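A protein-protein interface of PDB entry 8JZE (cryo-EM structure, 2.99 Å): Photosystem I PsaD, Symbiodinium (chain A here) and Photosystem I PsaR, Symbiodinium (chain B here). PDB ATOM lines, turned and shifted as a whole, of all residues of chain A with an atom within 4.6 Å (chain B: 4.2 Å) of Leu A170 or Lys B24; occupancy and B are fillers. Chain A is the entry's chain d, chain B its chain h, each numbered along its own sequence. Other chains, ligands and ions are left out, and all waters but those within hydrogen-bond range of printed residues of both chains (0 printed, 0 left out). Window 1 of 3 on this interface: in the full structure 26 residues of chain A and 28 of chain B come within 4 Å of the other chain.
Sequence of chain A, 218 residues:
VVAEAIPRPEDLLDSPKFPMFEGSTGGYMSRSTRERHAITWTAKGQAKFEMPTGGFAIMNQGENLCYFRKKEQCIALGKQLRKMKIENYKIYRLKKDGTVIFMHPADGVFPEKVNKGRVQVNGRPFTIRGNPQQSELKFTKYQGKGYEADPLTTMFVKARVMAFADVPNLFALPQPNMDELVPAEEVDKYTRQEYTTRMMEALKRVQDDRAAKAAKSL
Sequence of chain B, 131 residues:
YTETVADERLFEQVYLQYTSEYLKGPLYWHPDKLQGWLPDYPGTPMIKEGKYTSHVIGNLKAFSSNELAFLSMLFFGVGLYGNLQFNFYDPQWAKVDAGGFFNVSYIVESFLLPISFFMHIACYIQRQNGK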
ATOM      1  N   ALA A 163     -14.438  24.778  -3.893  1.00  0.00           N
ATOM      2  CA  ALA A 163     -15.082  23.518  -3.540  1.00  0.00           C
ATOM      3  C   ALA A 163     -14.676  23.053  -2.149  1.00  0.00           C
ATOM      4  O   ALA A 163     -15.524  22.644  -1.348  1.00  0.00           O
ATOM      5  CB  ALA A 163     -14.740  22.451  -4.579  1.00  0.00           C
ATOM      6  N   PHE A 164     -13.381  23.106  -1.839  1.00  0.00           N
ATOM      7  CA  PHE A 164     -12.891  22.541  -0.588  1.00  0.00           C
ATOM      8  C   PHE A 164     -13.052  23.534   0.557  1.00  0.00           C
ATOM      9  O   PHE A 164     -12.116  23.778   1.324  1.00  0.00           O
ATOM     10  CB  PHE A 164     -11.429  22.108  -0.734  1.00  0.00           C
ATOM     11  CG  PHE A 164     -11.228  20.944  -1.672  1.00  0.00           C
ATOM     12  CD1 PHE A 164     -12.310  20.209  -2.134  1.00  0.00           C
ATOM     13  CD2 PHE A 164      -9.957  20.582  -2.085  1.00  0.00           C
ATOM     14  CE1 PHE A 164     -12.127  19.142  -2.994  1.00  0.00           C
ATOM     15  CE2 PHE A 164      -9.767  19.514  -2.944  1.00  0.00           C
ATOM     16  CZ  PHE A 164     -10.854  18.794  -3.399  1.00  0.00           C
ATOM     17  N   ASP A 166     -16.868  23.784   1.463  1.00  0.00           N
ATOM     18  CA  ASP A 166     -18.135  23.169   1.844  1.00  0.00           C
ATOM     19  C   ASP A 166     -17.828  21.743   2.294  1.00  0.00           C
ATOM     20  O   ASP A 166     -18.038  20.762   1.579  1.00  0.00           O
ATOM     21  CB  ASP A 166     -19.118  23.216   0.681  1.00  0.00           C
ATOM     22  CG  ASP A 166     -20.518  22.809   1.081  1.00  0.00           C
ATOM     23  OD1 ASP A 166     -21.044  23.357   2.071  1.00  0.00           O
ATOM     24  OD2 ASP A 166     -21.102  21.951   0.388  1.00  0.00           O
ATOM     25  N   VAL A 167     -17.299  21.647   3.516  1.00  0.00           N
ATOM     26  CA  VAL A 167     -16.841  20.357   4.035  1.00  0.00           C
ATOM     27  C   VAL A 167     -17.956  19.317   4.116  1.00  0.00           C
ATOM     28  O   VAL A 167     -17.723  18.166   3.714  1.00  0.00           O
ATOM     29  CB  VAL A 167     -16.129  20.558   5.385  1.00  0.00           C
ATOM     30  CG1 VAL A 167     -15.774  19.221   6.009  1.00  0.00           C
ATOM     31  CG2 VAL A 167     -14.883  21.409   5.198  1.00  0.00           C
ATOM     32  N   PRO A 168     -19.159  19.629   4.622  1.00  0.00           N
ATOM     33  CA  PRO A 168     -20.161  18.562   4.805  1.00  0.00           C
ATOM     34  C   PRO A 168     -20.539  17.826   3.531  1.00  0.00           C
ATOM     35  O   PRO A 168     -20.888  16.641   3.599  1.00  0.00           O
ATOM     36  CB  PRO A 168     -21.365  19.313   5.392  1.00  0.00           C
ATOM     37  CG  PRO A 168     -20.778  20.486   6.063  1.00  0.00           C
ATOM     38  CD  PRO A 168     -19.627  20.901   5.202  1.00  0.00           C
ATOM     39  N   ASN A 169     -20.482  18.479   2.374  1.00  0.00           N
ATOM     40  CA  ASN A 169     -20.896  17.853   1.125  1.00  0.00           C
ATOM     41  C   ASN A 169     -19.747  17.217   0.355  1.00  0.00           C
ATOM     42  O   ASN A 169     -19.964  16.737  -0.762  1.00  0.00           O
ATOM     43  CB  ASN A 169     -21.604  18.874   0.229  1.00  0.00           C
ATOM     44  CG  ASN A 169     -22.814  19.497   0.897  1.00  0.00           C
ATOM     45  OD1 ASN A 169     -23.470  18.871   1.728  1.00  0.00           O
ATOM     46  ND2 ASN A 169     -23.114  20.738   0.535  1.00  0.00           N
ATOM     47  N   LEU A 170     -18.537  17.199   0.909  1.00  0.00           N
ATOM     48  CA  LEU A 170     -17.421  16.562   0.226  1.00  0.00           C
ATOM     49  C   LEU A 170     -17.599  15.046   0.202  1.00  0.00           C
ATOM     50  O   LEU A 170     -18.427  14.475   0.916  1.00  0.00           O
ATOM     51  CB  LEU A 170     -16.095  16.925   0.898  1.00  0.00           C
ATOM     52  CG  LEU A 170     -15.508  18.299   0.573  1.00  0.00           C
ATOM     53  CD1 LEU A 170     -14.136  18.464   1.202  1.00  0.00           C
ATOM     54  CD2 LEU A 170     -15.429  18.496  -0.927  1.00  0.00           C
ATOM     55  N   PHE A 171     -16.810  14.395  -0.649  1.00  0.00           N
ATOM     56  CA  PHE A 171     -16.803  12.942  -0.775  1.00  0.00           C
ATOM     57  C   PHE A 171     -15.456  12.425  -0.288  1.00  0.00           C
ATOM     58  O   PHE A 171     -14.423  12.687  -0.912  1.00  0.00           O
ATOM     59  CB  PHE A 171     -17.062  12.515  -2.218  1.00  0.00           C
ATOM     60  CG  PHE A 171     -16.803  11.057  -2.476  1.00  0.00           C
ATOM     61  CD1 PHE A 171     -17.746  10.103  -2.135  1.00  0.00           C
ATOM     62  CD2 PHE A 171     -15.618  10.643  -3.063  1.00  0.00           C
ATOM     63  CE1 PHE A 171     -17.512   8.762  -2.372  1.00  0.00           C
ATOM     64  CE2 PHE A 171     -15.378   9.304  -3.304  1.00  0.00           C
ATOM     65  CZ  PHE A 171     -16.327   8.362  -2.958  1.00  0.00           C
ATOM     66  N   ALA A 172     -15.466  11.693   0.821  1.00  0.00           N
ATOM     67  CA  ALA A 172     -14.242  11.086   1.318  1.00  0.00           C
ATOM     68  C   ALA A 172     -13.786   9.989   0.365  1.00  0.00           C
ATOM     69  O   ALA A 172     -14.590   9.168  -0.084  1.00  0.00           O
ATOM     70  CB  ALA A 172     -14.459  10.520   2.719  1.00  0.00           C
ATOM     71  N   SER B  20     -16.462  23.889  -9.246  1.00  0.00           N
ATOM     72  CA  SER B  20     -16.513  23.816  -7.789  1.00  0.00           C
ATOM     73  C   SER B  20     -17.556  22.814  -7.321  1.00  0.00           C
ATOM     74  O   SER B  20     -17.388  22.185  -6.271  1.00  0.00           O
ATOM     75  CB  SER B  20     -16.795  25.198  -7.202  1.00  0.00           C
ATOM     76  OG  SER B  20     -18.003  25.728  -7.718  1.00  0.00           O
ATOM     77  N   GLU B  21     -18.640  22.651  -8.080  1.00  0.00           N
ATOM     78  CA  GLU B  21     -19.611  21.612  -7.765  1.00  0.00           C
ATOM     79  C   GLU B  21     -19.109  20.235  -8.176  1.00  0.00           C
ATOM     80  O   GLU B  21     -19.376  19.244  -7.489  1.00  0.00           O
ATOM     81  CB  GLU B  21     -20.946  21.919  -8.445  1.00  0.00           C
ATOM     82  CG  GLU B  21     -21.689  23.096  -7.839  1.00  0.00           C
ATOM     83  CD  GLU B  21     -22.094  22.845  -6.402  1.00  0.00           C
ATOM     84  OE1 GLU B  21     -22.422  21.686  -6.071  1.00  0.00           O
ATOM     85  OE2 GLU B  21     -22.074  23.803  -5.601  1.00  0.00           O
ATOM     86  N   TYR B  22     -18.382  20.153  -9.293  1.00  0.00           N
ATOM     87  CA  TYR B  22     -17.910  18.857  -9.772  1.00  0.00           C
ATOM     88  C   TYR B  22     -16.843  18.271  -8.853  1.00  0.00           C
ATOM     89  O   TYR B  22     -16.821  17.058  -8.616  1.00  0.00           O
ATOM     90  CB  TYR B  22     -17.374  18.984 -11.198  1.00  0.00           C
ATOM     91  CG  TYR B  22     -16.995  17.664 -11.832  1.00  0.00           C
ATOM     92  CD1 TYR B  22     -17.944  16.889 -12.485  1.00  0.00           C
ATOM     93  CD2 TYR B  22     -15.689  17.194 -11.781  1.00  0.00           C
ATOM     94  CE1 TYR B  22     -17.606  15.684 -13.066  1.00  0.00           C
ATOM     95  CE2 TYR B  22     -15.341  15.990 -12.361  1.00  0.00           C
ATOM     96  CZ  TYR B  22     -16.303  15.240 -13.002  1.00  0.00           C
ATOM     97  OH  TYR B  22     -15.960  14.040 -13.579  1.00  0.00           O
ATOM     98  N   LEU B  23     -15.946  19.112  -8.335  1.00  0.00           N
ATOM     99  CA  LEU B  23     -14.819  18.610  -7.554  1.00  0.00           C
ATOM    100  C   LEU B  23     -15.265  18.060  -6.206  1.00  0.00           C
ATOM    101  O   LEU B  23     -14.576  17.213  -5.627  1.00  0.00           O
ATOM    102  CB  LEU B  23     -13.774  19.710  -7.360  1.00  0.00           C
ATOM    103  CG  LEU B  23     -13.192  20.328  -8.635  1.00  0.00           C
ATOM    104  CD1 LEU B  23     -12.036  21.259  -8.328  1.00  0.00           C
ATOM    105  CD2 LEU B  23     -12.769  19.259  -9.623  1.00  0.00           C
ATOM    106  N   LYS B  24     -16.403  18.525  -5.689  1.00  0.00           N
ATOM    107  CA  LYS B  24     -16.944  17.965  -4.457  1.00  0.00           C
ATOM    108  C   LYS B  24     -17.394  16.522  -4.632  1.00  0.00           C
ATOM    109  O   LYS B  24     -17.471  15.786  -3.643  1.00  0.00           O
ATOM    110  CB  LYS B  24     -18.119  18.810  -3.961  1.00  0.00           C
ATOM    111  CG  LYS B  24     -17.784  20.265  -3.687  1.00  0.00           C
ATOM    112  CD  LYS B  24     -19.046  21.068  -3.415  1.00  0.00           C
ATOM    113  CE  LYS B  24     -18.740  22.547  -3.242  1.00  0.00           C
ATOM    114  NZ  LYS B  24     -19.981  23.363  -3.132  1.00  0.00           N
ATOM    115  N   GLY B  25     -17.683  16.101  -5.859  1.00  0.00           N
ATOM    116  CA  GLY B  25     -18.253  14.800  -6.108  1.00  0.00           C
ATOM    117  C   GLY B  25     -17.237  13.680  -6.039  1.00  0.00           C
ATOM    118  O   GLY B  25     -16.077  13.875  -5.663  1.00  0.00           O
ATOM    119  N   LEU B  38      -9.772  17.237   4.831  1.00  0.00           N
ATOM    120  CA  LEU B  38     -10.984  18.046   4.977  1.00  0.00           C
ATOM    121  C   LEU B  38     -12.278  17.244   5.082  1.00  0.00           C
ATOM    122  O   LEU B  38     -13.043  17.488   6.027  1.00  0.00           O
ATOM    123  CB  LEU B  38     -11.060  19.031   3.802  1.00  0.00           C
ATOM    124  CG  LEU B  38      -9.819  19.882   3.534  1.00  0.00           C
ATOM    125  CD1 LEU B  38      -9.898  20.525   2.163  1.00  0.00           C
ATOM    126  CD2 LEU B  38      -9.659  20.941   4.607  1.00  0.00           C
ATOM    127  N   PRO B  39     -12.589  16.296   4.192  1.00  0.00           N
ATOM    128  CA  PRO B  39     -13.911  15.660   4.252  1.00  0.00           C
ATOM    129  C   PRO B  39     -14.079  14.795   5.490  1.00  0.00           C
ATOM    130  O   PRO B  39     -13.117  14.243   6.032  1.00  0.00           O
ATOM    131  CB  PRO B  39     -13.954  14.812   2.976  1.00  0.00           C
ATOM    132  CG  PRO B  39     -12.544  14.487   2.715  1.00  0.00           C
ATOM    133  CD  PRO B  39     -11.770  15.713   3.114  1.00  0.00           C
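The backbone NH (N) of Phe A171 lies within hydrogen-bond range of the backbone carbonyl oxygen (O) of Lys B24 (3.4 Å).
The side-chain amino group (NZ) of Lys B24 lies within salt-bridge range of the side-chain carboxylate (OD2) of Asp A166 (3.95 Å).
The side-chain amino group of Lys B24 lies within salt-bridge range of the side-chain carboxylate of Glu B21 (3.3 Å).
Among the printed residues, pairs that only touch across the chains: Ala A163 with Ser B20, Ala A163 with Lys B24, Phe A164 with Leu B38, Val A167 with Leu B38, Asn A169 with Lys B24, Leu A170 with Lys B24, Leu A170 with Pro B39 and Phe A171 with Gly B25.
Printed residues of chain B within 4 Å of Ala A163: Ser B20 (3.2 Å) and Lys B24 (3.7 Å).
Leu A170 touches just these residues of chain B: Lys B24 and Pro B39.
Of chain A, only Ala A163, Asp A166, Asn A169, Leu A170 and Phe A171 come within 4 Å of Lys B24.
Printed residues of chain A within 4 Å of Pro B39: Leu A170.
The nearest residue of chain B that does not touch Leu A170 is Leu B38 (4.1 Å).
The nearest printed residue of chain A that does not touch Pro B39 is Ala A172 (4.05 Å).
Of the 8 printed residues of chain B, 5 touch a printed residue of chain A.
Printed residues of chain B that touch a printed residue of chain A: Ser B20, Lys B24, Gly B25, Leu B38 and Pro B39.
Hydrophobic or aromatic side chains of chain B within 4 Å of the printed part of chain A: Leu B38 and Pro B39.
Along chain B the printed residues that touch a printed residue of chain A span positions 20 to 39.
Among the printed residues, Asp or Glu carboxylates within 4 Å of a Lys or Arg side-chain nitrogen of the other chain: Asp A166 with Lys B24.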
